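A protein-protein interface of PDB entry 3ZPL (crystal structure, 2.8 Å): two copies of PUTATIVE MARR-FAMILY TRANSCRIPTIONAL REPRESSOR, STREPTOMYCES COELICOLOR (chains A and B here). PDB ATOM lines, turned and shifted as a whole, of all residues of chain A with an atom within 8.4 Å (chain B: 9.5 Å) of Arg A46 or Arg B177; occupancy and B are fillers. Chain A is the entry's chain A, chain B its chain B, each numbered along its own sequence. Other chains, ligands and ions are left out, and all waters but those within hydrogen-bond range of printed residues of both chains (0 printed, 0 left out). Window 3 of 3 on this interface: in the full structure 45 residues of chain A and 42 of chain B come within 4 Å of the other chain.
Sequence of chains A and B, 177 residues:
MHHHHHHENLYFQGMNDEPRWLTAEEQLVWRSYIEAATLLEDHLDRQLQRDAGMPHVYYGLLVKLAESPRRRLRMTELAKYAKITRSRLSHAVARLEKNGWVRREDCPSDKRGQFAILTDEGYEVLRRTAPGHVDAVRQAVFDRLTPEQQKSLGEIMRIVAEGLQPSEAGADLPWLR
Arg A46 touches just these residues of chain B: Asp B172 (3.2 Å) and Arg B177 (3.3 Å).
Arg B177 touches two residues of chain A.
No residue of chain B comes within 4 Å of Asp A45.
No residue of chain B comes within 4 Å of Gln A49.
Printed residues of chain A within 4 Å of Pro B174: Asp A42 (3.9 Å).
Printed residues of chain B within 4 Å of Asp A42: Pro B174 and Arg B177.
Of the printed residues of chain B, Leu A39 touches Lys B83.
Printed residues of chain B within 4 Å of Leu A40: Leu B164 (3.8 Å).
Of the printed residues of chain A, Leu B164 touches Leu A40 (3.8 Å) and His A43 (3.4 Å).
Printed residues of chain A within 4 Å of Lys B83: Thr A38 (3.8 Å) and Leu A39 (3.9 Å).
The nearest residue of chain B that does not touch Arg A46 is Thr B85 (6.9 Å).
The nearest residue of chain A that does not touch Arg B177 is His A43 (6.2 Å).
Of the 20 printed residues of chain A, 6 touch a printed residue of chain B.
Hydrophobic or aromatic side chains of chain A that line the printed part of chain B: Leu A39, Leu A40 and His A43.
Among the printed residues, 8 pairs touch across the chains.
Among the printed residues, Asp or Glu carboxylates within 4 Å of a Lys or Arg side-chain nitrogen of the other chain: Asp A42 with Arg B177 (2.8 Å) and Arg A46 with Asp B172 (3.2 Å).
The side-chain carboxylate (OD1) of Asp B172 is in salt-bridge range of the guanidinium group (NH1) of Arg B177.
The guanidinium group of Arg B86 is in salt-bridge range of the chain-end carboxylate of Arg B177, 3.9 Å away.
The side-chain carboxylate (OD2) of Asp A42 lies within salt-bridge range of the guanidinium group (NH2) of Arg B177, 2.8 Å away.
NE of Arg B177 sits close to NH1 of Arg A46 (3.3 Å).
The side-chain carboxylate (OD2) of Asp B172 lies within salt-bridge range of the guanidinium group (NH1) of Arg A46, at 3.2 Å.
No position is printed for both chains.
Of the 8 pairs that touch across the chains among the printed residues, none has its exchanged pair printed and touching as well.
Among the printed residues, pairs that only touch across the chains: Thr A38 with Lys B83 (3.8 Å), Leu A39 with Lys B83 (3.9 Å), Leu A40 with Leu B164 (3.8 Å), Asp A42 with Pro B174 (3.9 Å) and His A43 with Leu B164 (3.4 Å).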
ATOM      1  N   THR A  38      -7.350 -19.598 -14.800  1.00  0.00           N
ATOM      2  CA  THR A  38      -7.322 -20.814 -15.601  1.00  0.00           C
ATOM      3  C   THR A  38      -8.058 -21.927 -14.875  1.00  0.00           C
ATOM      4  O   THR A  38      -8.682 -22.765 -15.533  1.00  0.00           O
ATOM      5  CB  THR A  38      -5.888 -21.267 -15.935  1.00  0.00           C
ATOM      6  OG1 THR A  38      -5.156 -20.186 -16.517  1.00  0.00           O
ATOM      7  CG2 THR A  38      -5.892 -22.449 -16.918  1.00  0.00           C
ATOM      8  N   LEU A  39      -8.012 -21.929 -13.535  1.00  0.00           N
ATOM      9  CA  LEU A  39      -8.698 -22.949 -12.726  1.00  0.00           C
ATOM     10  C   LEU A  39     -10.193 -22.679 -12.642  1.00  0.00           C
ATOM     11  O   LEU A  39     -10.982 -23.612 -12.675  1.00  0.00           O
ATOM     12  CB  LEU A  39      -8.127 -23.034 -11.301  1.00  0.00           C
ATOM     13  CG  LEU A  39      -6.740 -23.660 -11.109  1.00  0.00           C
ATOM     14  CD1 LEU A  39      -6.219 -23.299  -9.744  1.00  0.00           C
ATOM     15  CD2 LEU A  39      -6.750 -25.169 -11.287  1.00  0.00           C
ATOM     16  N   LEU A  40     -10.578 -21.411 -12.493  1.00  0.00           N
ATOM     17  CA  LEU A  40     -11.992 -21.051 -12.519  1.00  0.00           C
ATOM     18  C   LEU A  40     -12.666 -21.423 -13.856  1.00  0.00           C
ATOM     19  O   LEU A  40     -13.689 -22.109 -13.853  1.00  0.00           O
ATOM     20  CB  LEU A  40     -12.196 -19.560 -12.263  1.00  0.00           C
ATOM     21  CG  LEU A  40     -12.755 -19.174 -10.907  1.00  0.00           C
ATOM     22  CD1 LEU A  40     -12.886 -17.658 -10.826  1.00  0.00           C
ATOM     23  CD2 LEU A  40     -14.102 -19.846 -10.627  1.00  0.00           C
ATOM     24  N   GLU A  41     -12.111 -20.968 -14.981  1.00  0.00           N
ATOM     25  CA  GLU A  41     -12.706 -21.299 -16.294  1.00  0.00           C
ATOM     26  C   GLU A  41     -12.827 -22.810 -16.406  1.00  0.00           C
ATOM     27  O   GLU A  41     -13.808 -23.298 -16.920  1.00  0.00           O
ATOM     28  CB  GLU A  41     -11.954 -20.742 -17.508  1.00  0.00           C
ATOM     29  N   ASP A  42     -11.843 -23.544 -15.888  1.00  0.00           N
ATOM     30  CA  ASP A  42     -11.885 -24.995 -15.947  1.00  0.00           C
ATOM     31  C   ASP A  42     -13.014 -25.558 -15.082  1.00  0.00           C
ATOM     32  O   ASP A  42     -13.770 -26.428 -15.503  1.00  0.00           O
ATOM     33  CB  ASP A  42     -10.545 -25.565 -15.495  1.00  0.00           C
ATOM     34  CG  ASP A  42     -10.508 -27.065 -15.544  1.00  0.00           C
ATOM     35  OD1 ASP A  42     -10.897 -27.710 -14.558  1.00  0.00           O
ATOM     36  OD2 ASP A  42     -10.101 -27.617 -16.578  1.00  0.00           O
ATOM     37  N   HIS A  43     -13.105 -25.055 -13.861  1.00  0.00           N
ATOM     38  CA  HIS A  43     -14.066 -25.551 -12.905  1.00  0.00           C
ATOM     39  C   HIS A  43     -15.485 -25.267 -13.387  1.00  0.00           C
ATOM     40  O   HIS A  43     -16.365 -26.146 -13.320  1.00  0.00           O
ATOM     41  CB  HIS A  43     -13.810 -24.927 -11.536  1.00  0.00           C
ATOM     42  CG  HIS A  43     -14.784 -25.359 -10.492  1.00  0.00           C
ATOM     43  ND1 HIS A  43     -15.053 -26.683 -10.229  1.00  0.00           N
ATOM     44  CD2 HIS A  43     -15.572 -24.639  -9.658  1.00  0.00           C
ATOM     45  CE1 HIS A  43     -15.955 -26.761  -9.264  1.00  0.00           C
ATOM     46  NE2 HIS A  43     -16.290 -25.533  -8.905  1.00  0.00           N
ATOM     47  N   LEU A  44     -15.693 -24.062 -13.906  1.00  0.00           N
ATOM     48  CA  LEU A  44     -17.025 -23.634 -14.318  1.00  0.00           C
ATOM     49  C   LEU A  44     -17.448 -24.257 -15.640  1.00  0.00           C
ATOM     50  O   LEU A  44     -18.569 -24.749 -15.755  1.00  0.00           O
ATOM     51  CB  LEU A  44     -17.103 -22.109 -14.380  1.00  0.00           C
ATOM     52  CG  LEU A  44     -16.824 -21.430 -13.034  1.00  0.00           C
ATOM     53  CD1 LEU A  44     -17.127 -19.939 -13.105  1.00  0.00           C
ATOM     54  CD2 LEU A  44     -17.609 -22.078 -11.910  1.00  0.00           C
ATOM     55  N   ASP A  45     -16.556 -24.256 -16.628  1.00  0.00           N
ATOM     56  CA  ASP A  45     -16.787 -24.988 -17.876  1.00  0.00           C
ATOM     57  C   ASP A  45     -17.227 -26.412 -17.594  1.00  0.00           C
ATOM     58  O   ASP A  45     -18.146 -26.899 -18.220  1.00  0.00           O
ATOM     59  CB  ASP A  45     -15.534 -25.063 -18.742  1.00  0.00           C
ATOM     60  CG  ASP A  45     -15.350 -23.850 -19.655  1.00  0.00           C
ATOM     61  OD1 ASP A  45     -16.239 -22.971 -19.721  1.00  0.00           O
ATOM     62  OD2 ASP A  45     -14.285 -23.810 -20.325  1.00  0.00           O
ATOM     63  N   ARG A  46     -16.554 -27.090 -16.677  1.00  0.00           N
ATOM     64  CA  ARG A  46     -16.879 -28.487 -16.407  1.00  0.00           C
ATOM     65  C   ARG A  46     -18.223 -28.637 -15.716  1.00  0.00           C
ATOM     66  O   ARG A  46     -18.999 -29.527 -16.030  1.00  0.00           O
ATOM     67  CB  ARG A  46     -15.797 -29.133 -15.541  1.00  0.00           C
ATOM     68  CG  ARG A  46     -14.512 -29.398 -16.296  1.00  0.00           C
ATOM     69  CD  ARG A  46     -13.820 -30.643 -15.795  1.00  0.00           C
ATOM     70  NE  ARG A  46     -13.964 -31.701 -16.786  1.00  0.00           N
ATOM     71  CZ  ARG A  46     -13.758 -32.984 -16.543  1.00  0.00           C
ATOM     72  NH1 ARG A  46     -13.399 -33.387 -15.329  1.00  0.00           N
ATOM     73  NH2 ARG A  46     -13.915 -33.871 -17.515  1.00  0.00           N
ATOM     74  N   GLN A  47     -18.451 -27.800 -14.713  1.00  0.00           N
ATOM     75  CA  GLN A  47     -19.708 -27.785 -14.004  1.00  0.00           C
ATOM     76  C   GLN A  47     -20.858 -27.577 -15.003  1.00  0.00           C
ATOM     77  O   GLN A  47     -21.868 -28.278 -14.953  1.00  0.00           O
ATOM     78  CB  GLN A  47     -19.677 -26.680 -12.943  1.00  0.00           C
ATOM     79  CG  GLN A  47     -20.916 -26.601 -12.069  1.00  0.00           C
ATOM     80  CD  GLN A  47     -21.921 -25.603 -12.594  1.00  0.00           C
ATOM     81  OE1 GLN A  47     -21.559 -24.478 -12.945  1.00  0.00           O
ATOM     82  NE2 GLN A  47     -23.190 -26.010 -12.669  1.00  0.00           N
ATOM     83  N   LEU A  48     -20.684 -26.639 -15.928  1.00  0.00           N
ATOM     84  CA  LEU A  48     -21.735 -26.345 -16.899  1.00  0.00           C
ATOM     85  C   LEU A  48     -21.815 -27.360 -18.035  1.00  0.00           C
ATOM     86  O   LEU A  48     -22.882 -27.598 -18.561  1.00  0.00           O
ATOM     87  CB  LEU A  48     -21.573 -24.946 -17.454  1.00  0.00           C
ATOM     88  CG  LEU A  48     -21.990 -23.899 -16.434  1.00  0.00           C
ATOM     89  CD1 LEU A  48     -21.379 -22.543 -16.755  1.00  0.00           C
ATOM     90  CD2 LEU A  48     -23.502 -23.799 -16.360  1.00  0.00           C
ATOM     91  N   GLN A  49     -20.701 -27.981 -18.395  1.00  0.00           N
ATOM     92  CA  GLN A  49     -20.713 -29.004 -19.438  1.00  0.00           C
ATOM     93  C   GLN A  49     -21.466 -30.263 -18.978  1.00  0.00           C
ATOM     94  O   GLN A  49     -22.174 -30.886 -19.782  1.00  0.00           O
ATOM     95  CB  GLN A  49     -19.284 -29.352 -19.909  1.00  0.00           C
ATOM     96  N   ARG A  50     -21.332 -30.643 -17.706  1.00  0.00           N
ATOM     97  CA  ARG A  50     -22.048 -31.821 -17.203  1.00  0.00           C
ATOM     98  C   ARG A  50     -23.494 -31.508 -16.849  1.00  0.00           C
ATOM     99  O   ARG A  50     -24.388 -32.214 -17.280  1.00  0.00           O
ATOM    100  CB  ARG A  50     -21.361 -32.434 -15.971  1.00  0.00           C
ATOM    101  N   ASP A  51     -23.712 -30.459 -16.057  1.00  0.00           N
ATOM    102  CA  ASP A  51     -25.035 -30.148 -15.505  1.00  0.00           C
ATOM    103  C   ASP A  51     -25.971 -29.447 -16.484  1.00  0.00           C
ATOM    104  O   ASP A  51     -27.174 -29.409 -16.261  1.00  0.00           O
ATOM    105  CB  ASP A  51     -24.909 -29.285 -14.239  1.00  0.00           C
ATOM    106  CG  ASP A  51     -24.074 -29.944 -13.147  1.00  0.00           C
ATOM    107  OD1 ASP A  51     -23.722 -31.138 -13.276  1.00  0.00           O
ATOM    108  OD2 ASP A  51     -23.754 -29.268 -12.151  1.00  0.00           O
ATOM    109  N   ALA A  52     -25.435 -28.914 -17.573  1.00  0.00           N
ATOM    110  CA  ALA A  52     -26.243 -28.133 -18.534  1.00  0.00           C
ATOM    111  C   ALA A  52     -25.896 -28.340 -20.022  1.00  0.00           C
ATOM    112  O   ALA A  52     -26.544 -27.779 -20.890  1.00  0.00           O
ATOM    113  CB  ALA A  52     -26.135 -26.658 -18.182  1.00  0.00           C
ATOM    114  N   GLY A  53     -24.857 -29.112 -20.314  1.00  0.00           N
ATOM    115  CA  GLY A  53     -24.525 -29.460 -21.690  1.00  0.00           C
ATOM    116  C   GLY A  53     -23.930 -28.352 -22.534  1.00  0.00           C
ATOM    117  O   GLY A  53     -24.001 -28.422 -23.745  1.00  0.00           O
ATOM    118  N   MET A  54     -23.301 -27.351 -21.916  1.00  0.00           N
ATOM    119  CA  MET A  54     -22.640 -26.276 -22.672  1.00  0.00           C
ATOM    120  C   MET A  54     -21.559 -25.583 -21.863  1.00  0.00           C
ATOM    121  O   MET A  54     -21.595 -25.617 -20.633  1.00  0.00           O
ATOM    122  CB  MET A  54     -23.662 -25.254 -23.106  1.00  0.00           C
ATOM    123  CG  MET A  54     -24.116 -24.323 -22.009  1.00  0.00           C
ATOM    124  SD  MET A  54     -25.500 -23.369 -22.630  1.00  0.00           S
ATOM    125  CE  MET A  54     -26.529 -23.299 -21.162  1.00  0.00           C
ATOM    126  N   PRO A  55     -20.599 -24.932 -22.549  1.00  0.00           N
ATOM    127  CA  PRO A  55     -19.490 -24.264 -21.881  1.00  0.00           C
ATOM    128  C   PRO A  55     -19.884 -22.943 -21.269  1.00  0.00           C
ATOM    129  O   PRO A  55     -20.975 -22.472 -21.487  1.00  0.00           O
ATOM    130  CB  PRO A  55     -18.495 -24.046 -23.003  1.00  0.00           C
ATOM    131  CG  PRO A  55     -19.357 -23.858 -24.198  1.00  0.00           C
ATOM    132  CD  PRO A  55     -20.494 -24.813 -24.010  1.00  0.00           C
ATOM    133  N   HIS A  56     -19.001 -22.357 -20.472  1.00  0.00           N
ATOM    134  CA  HIS A  56     -19.355 -21.162 -19.699  1.00  0.00           C
ATOM    135  C   HIS A  56     -19.743 -19.989 -20.575  1.00  0.00           C
ATOM    136  O   HIS A  56     -20.661 -19.256 -20.245  1.00  0.00           O
ATOM    137  CB  HIS A  56     -18.230 -20.754 -18.750  1.00  0.00           C
ATOM    138  CG  HIS A  56     -18.608 -19.645 -17.812  1.00  0.00           C
ATOM    139  ND1 HIS A  56     -17.716 -18.674 -17.408  1.00  0.00           N
ATOM    140  CD2 HIS A  56     -19.774 -19.358 -17.183  1.00  0.00           C
ATOM    141  CE1 HIS A  56     -18.308 -17.848 -16.562  1.00  0.00           C
ATOM    142  NE2 HIS A  56     -19.558 -18.240 -16.407  1.00  0.00           N
ATOM    143  N   ALA A 136     -21.648 -23.121  -7.509  1.00  0.00           N
ATOM    144  CA  ALA A 136     -20.266 -23.298  -7.964  1.00  0.00           C
ATOM    145  C   ALA A 136     -19.477 -21.980  -7.966  1.00  0.00           C
ATOM    146  O   ALA A 136     -18.311 -21.951  -7.580  1.00  0.00           O
ATOM    147  CB  ALA A 136     -20.237 -23.936  -9.349  1.00  0.00           C
ATOM    148  N   THR B  76       3.605 -34.175 -16.268  1.00  0.00           N
ATOM    149  CA  THR B  76       2.579 -33.920 -15.280  1.00  0.00           C
ATOM    150  C   THR B  76       2.930 -32.686 -14.446  1.00  0.00           C
ATOM    151  O   THR B  76       2.047 -31.886 -14.145  1.00  0.00           O
ATOM    152  CB  THR B  76       2.327 -35.138 -14.369  1.00  0.00           C
ATOM    153  OG1 THR B  76       1.962 -36.280 -15.160  1.00  0.00           O
ATOM    154  CG2 THR B  76       1.201 -34.844 -13.407  1.00  0.00           C
ATOM    155  N   ALA B  79       2.064 -29.706 -16.471  1.00  0.00           N
ATOM    156  CA  ALA B  79       0.620 -29.515 -16.435  1.00  0.00           C
ATOM    157  C   ALA B  79       0.165 -28.902 -15.113  1.00  0.00           C
ATOM    158  O   ALA B  79      -0.690 -28.029 -15.114  1.00  0.00           O
ATOM    159  CB  ALA B  79      -0.077 -30.836 -16.674  1.00  0.00           C
ATOM    160  N   LYS B  83      -1.790 -25.561 -14.777  1.00  0.00           N
ATOM    161  CA  LYS B  83      -3.177 -25.797 -14.370  1.00  0.00           C
ATOM    162  C   LYS B  83      -4.040 -26.296 -15.534  1.00  0.00           C
ATOM    163  O   LYS B  83      -5.227 -25.992 -15.614  1.00  0.00           O
ATOM    164  CB  LYS B  83      -3.801 -24.554 -13.739  1.00  0.00           C
ATOM    165  CG  LYS B  83      -2.921 -23.868 -12.701  1.00  0.00           C
ATOM    166  CD  LYS B  83      -2.683 -24.746 -11.495  1.00  0.00           C
ATOM    167  CE  LYS B  83      -1.493 -24.257 -10.700  1.00  0.00           C
ATOM    168  NZ  LYS B  83      -1.189 -25.152  -9.552  1.00  0.00           N
ATOM    169  N   ILE B  84      -3.437 -27.099 -16.401  1.00  0.00           N
ATOM    170  CA  ILE B  84      -4.109 -27.630 -17.557  1.00  0.00           C
ATOM    171  C   ILE B  84      -4.066 -29.142 -17.481  1.00  0.00           C
ATOM    172  O   ILE B  84      -3.517 -29.686 -16.533  1.00  0.00           O
ATOM    173  CB  ILE B  84      -3.447 -27.170 -18.857  1.00  0.00           C
ATOM    174  CG1 ILE B  84      -2.113 -27.881 -19.067  1.00  0.00           C
ATOM    175  CG2 ILE B  84      -3.314 -25.655 -18.870  1.00  0.00           C
ATOM    176  CD1 ILE B  84      -1.247 -27.287 -20.159  1.00  0.00           C
ATOM    177  N   THR B  85      -4.689 -29.820 -18.444  1.00  0.00           N
ATOM    178  CA  THR B  85      -4.696 -31.266 -18.420  1.00  0.00           C
ATOM    179  C   THR B  85      -3.504 -31.803 -19.169  1.00  0.00           C
ATOM    180  O   THR B  85      -2.941 -31.147 -20.025  1.00  0.00           O
ATOM    181  CB  THR B  85      -5.974 -31.855 -19.029  1.00  0.00           C
ATOM    182  OG1 THR B  85      -6.034 -31.546 -20.428  1.00  0.00           O
ATOM    183  CG2 THR B  85      -7.205 -31.320 -18.304  1.00  0.00           C
ATOM    184  N   ARG B  86      -3.121 -33.018 -18.825  1.00  0.00           N
ATOM    185  CA  ARG B  86      -2.045 -33.716 -19.508  1.00  0.00           C
ATOM    186  C   ARG B  86      -2.296 -33.799 -21.009  1.00  0.00           C
ATOM    187  O   ARG B  86      -1.349 -33.833 -21.800  1.00  0.00           O
ATOM    188  CB  ARG B  86      -1.923 -35.129 -18.955  1.00  0.00           C
ATOM    189  CG  ARG B  86      -1.578 -35.171 -17.486  1.00  0.00           C
ATOM    190  CD  ARG B  86      -1.496 -36.596 -17.043  1.00  0.00           C
ATOM    191  NE  ARG B  86      -1.033 -36.726 -15.672  1.00  0.00           N
ATOM    192  CZ  ARG B  86      -1.353 -37.728 -14.862  1.00  0.00           C
ATOM    193  NH1 ARG B  86      -2.178 -38.683 -15.272  1.00  0.00           N
ATOM    194  NH2 ARG B  86      -0.849 -37.774 -13.639  1.00  0.00           N
ATOM    195  N   SER B  87      -3.575 -33.898 -21.374  1.00  0.00           N
ATOM    196  CA  SER B  87      -3.992 -34.136 -22.745  1.00  0.00           C
ATOM    197  C   SER B  87      -3.680 -32.912 -23.535  1.00  0.00           C
ATOM    198  O   SER B  87      -2.998 -32.945 -24.568  1.00  0.00           O
ATOM    199  CB  SER B  87      -5.487 -34.361 -22.778  1.00  0.00           C
ATOM    200  OG  SER B  87      -5.779 -35.538 -23.470  1.00  0.00           O
ATOM    201  N   ARG B  88      -4.179 -31.794 -23.018  1.00  0.00           N
ATOM    202  CA  ARG B  88      -3.908 -30.510 -23.600  1.00  0.00           C
ATOM    203  C   ARG B  88      -2.404 -30.288 -23.681  1.00  0.00           C
ATOM    204  O   ARG B  88      -1.912 -29.777 -24.678  1.00  0.00           O
ATOM    205  CB  ARG B  88      -4.548 -29.435 -22.757  1.00  0.00           C
ATOM    206  CG  ARG B  88      -4.380 -28.034 -23.333  1.00  0.00           C
ATOM    207  CD  ARG B  88      -4.906 -27.051 -22.320  1.00  0.00           C
ATOM    208  NE  ARG B  88      -5.080 -25.729 -22.863  1.00  0.00           N
ATOM    209  CZ  ARG B  88      -5.754 -24.772 -22.232  1.00  0.00           C
ATOM    210  NH1 ARG B  88      -6.299 -25.011 -21.046  1.00  0.00           N
ATOM    211  NH2 ARG B  88      -5.883 -23.578 -22.785  1.00  0.00           N
ATOM    212  N   LEU B 164      -9.582 -23.990  -5.316  1.00  0.00           N
ATOM    213  CA  LEU B 164      -9.937 -24.834  -6.451  1.00  0.00           C
ATOM    214  C   LEU B 164      -8.972 -25.983  -6.642  1.00  0.00           C
ATOM    215  O   LEU B 164      -9.192 -26.849  -7.487  1.00  0.00           O
ATOM    216  CB  LEU B 164      -9.998 -23.992  -7.728  1.00  0.00           C
ATOM    217  CG  LEU B 164     -11.278 -23.179  -7.875  1.00  0.00           C
ATOM    218  CD1 LEU B 164     -11.037 -21.940  -8.721  1.00  0.00           C
ATOM    219  CD2 LEU B 164     -12.373 -24.056  -8.468  1.00  0.00           C
ATOM    220  N   GLY B 170      -9.663 -37.451  -3.796  1.00  0.00           N
ATOM    221  CA  GLY B 170     -10.211 -37.833  -5.100  1.00  0.00           C
ATOM    222  C   GLY B 170     -10.635 -36.628  -5.931  1.00  0.00           C
ATOM    223  O   GLY B 170     -11.549 -36.751  -6.749  1.00  0.00           O
ATOM    224  N   ALA B 171      -9.991 -35.469  -5.716  1.00  0.00           N
ATOM    225  CA  ALA B 171     -10.455 -34.184  -6.334  1.00  0.00           C
ATOM    226  C   ALA B 171     -10.165 -34.115  -7.836  1.00  0.00           C
ATOM    227  O   ALA B 171      -9.317 -34.849  -8.370  1.00  0.00           O
ATOM    228  CB  ALA B 171      -9.892 -32.938  -5.613  1.00  0.00           C
ATOM    229  N   ASP B 172     -10.860 -33.201  -8.505  1.00  0.00           N
ATOM    230  CA  ASP B 172     -10.956 -33.184  -9.956  1.00  0.00           C
ATOM    231  C   ASP B 172      -9.949 -32.191 -10.543  1.00  0.00           C
ATOM    232  O   ASP B 172     -10.316 -31.264 -11.265  1.00  0.00           O
ATOM    233  CB  ASP B 172     -12.394 -32.836 -10.371  1.00  0.00           C
ATOM    234  CG  ASP B 172     -12.598 -32.912 -11.866  1.00  0.00           C
ATOM    235  OD1 ASP B 172     -11.800 -33.608 -12.534  1.00  0.00           O
ATOM    236  OD2 ASP B 172     -13.532 -32.264 -12.386  1.00  0.00           O
ATOM    237  N   LEU B 173      -8.675 -32.383 -10.214  1.00  0.00           N
ATOM    238  CA  LEU B 173      -7.629 -31.481 -10.671  1.00  0.00           C
ATOM    239  C   LEU B 173      -7.250 -31.841 -12.098  1.00  0.00           C
ATOM    240  O   LEU B 173      -7.046 -33.021 -12.398  1.00  0.00           O
ATOM    241  CB  LEU B 173      -6.408 -31.566  -9.743  1.00  0.00           C
ATOM    242  CG  LEU B 173      -6.698 -31.356  -8.245  1.00  0.00           C
ATOM    243  CD1 LEU B 173      -5.468 -31.569  -7.379  1.00  0.00           C
ATOM    244  CD2 LEU B 173      -7.282 -29.979  -7.982  1.00  0.00           C
ATOM    245  N   PRO B 174      -7.163 -30.834 -12.988  1.00  0.00           N
ATOM    246  CA  PRO B 174      -6.898 -31.039 -14.428  1.00  0.00           C
ATOM    247  C   PRO B 174      -5.779 -32.040 -14.725  1.00  0.00           C
ATOM    248  O   PRO B 174      -5.925 -32.916 -15.571  1.00  0.00           O
ATOM    249  CB  PRO B 174      -6.485 -29.641 -14.911  1.00  0.00           C
ATOM    250  CG  PRO B 174      -7.140 -28.701 -13.969  1.00  0.00           C
ATOM    251  CD  PRO B 174      -7.289 -29.405 -12.654  1.00  0.00           C
ATOM    252  N   TRP B 175      -4.667 -31.892 -14.026  1.00  0.00           N
ATOM    253  CA  TRP B 175      -3.475 -32.681 -14.312  1.00  0.00           C
ATOM    254  C   TRP B 175      -3.570 -34.117 -13.786  1.00  0.00           C
ATOM    255  O   TRP B 175      -2.731 -34.955 -14.109  1.00  0.00           O
ATOM    256  CB  TRP B 175      -2.243 -31.992 -13.755  1.00  0.00           C
ATOM    257  CG  TRP B 175      -2.333 -31.658 -12.309  1.00  0.00           C
ATOM    258  CD1 TRP B 175      -1.874 -32.404 -11.269  1.00  0.00           C
ATOM    259  CD2 TRP B 175      -2.894 -30.478 -11.740  1.00  0.00           C
ATOM    260  NE1 TRP B 175      -2.116 -31.764 -10.083  1.00  0.00           N
ATOM    261  CE2 TRP B 175      -2.738 -30.575 -10.346  1.00  0.00           C
ATOM    262  CE3 TRP B 175      -3.516 -29.352 -12.269  1.00  0.00           C
ATOM    263  CZ2 TRP B 175      -3.185 -29.601  -9.479  1.00  0.00           C
ATOM    264  CZ3 TRP B 175      -3.952 -28.368 -11.398  1.00  0.00           C
ATOM    265  CH2 TRP B 175      -3.785 -28.500 -10.022  1.00  0.00           C
ATOM    266  N   LEU B 176      -4.607 -34.394 -12.995  1.00  0.00           N
ATOM    267  CA  LEU B 176      -4.932 -35.760 -12.578  1.00  0.00           C
ATOM    268  C   LEU B 176      -6.096 -36.343 -13.369  1.00  0.00           C
ATOM    269  O   LEU B 176      -6.621 -37.394 -13.021  1.00  0.00           O
ATOM    270  CB  LEU B 176      -5.234 -35.794 -11.082  1.00  0.00           C
ATOM    271  CG  LEU B 176      -4.147 -35.230 -10.177  1.00  0.00           C
ATOM    272  CD1 LEU B 176      -4.597 -35.372  -8.733  1.00  0.00           C
ATOM    273  CD2 LEU B 176      -2.816 -35.922 -10.414  1.00  0.00           C
ATOM    274  N   ARG B 177      -6.482 -35.680 -14.448  1.00  0.00           N
ATOM    275  CA  ARG B 177      -7.576 -36.164 -15.268  1.00  0.00           C
ATOM    276  C   ARG B 177      -7.002 -37.267 -16.141  1.00  0.00           C
ATOM    277  O   ARG B 177      -5.816 -37.610 -16.006  1.00  0.00           O
ATOM    278  CB  ARG B 177      -8.156 -35.052 -16.151  1.00  0.00           C
ATOM    279  CG  ARG B 177      -9.664 -34.951 -16.088  1.00  0.00           C
ATOM    280  CD  ARG B 177     -10.087 -33.866 -15.125  1.00  0.00           C
ATOM    281  NE  ARG B 177     -10.196 -32.584 -15.803  1.00  0.00           N
ATOM    282  CZ  ARG B 177     -10.428 -31.415 -15.204  1.00  0.00           C
ATOM    283  NH1 ARG B 177     -10.573 -31.332 -13.892  1.00  0.00           N
ATOM    284  NH2 ARG B 177     -10.501 -30.312 -15.935  1.00  0.00           N
ATOM    285  OXT ARG B 177      -7.698 -37.836 -16.974  1.00  0.00           O
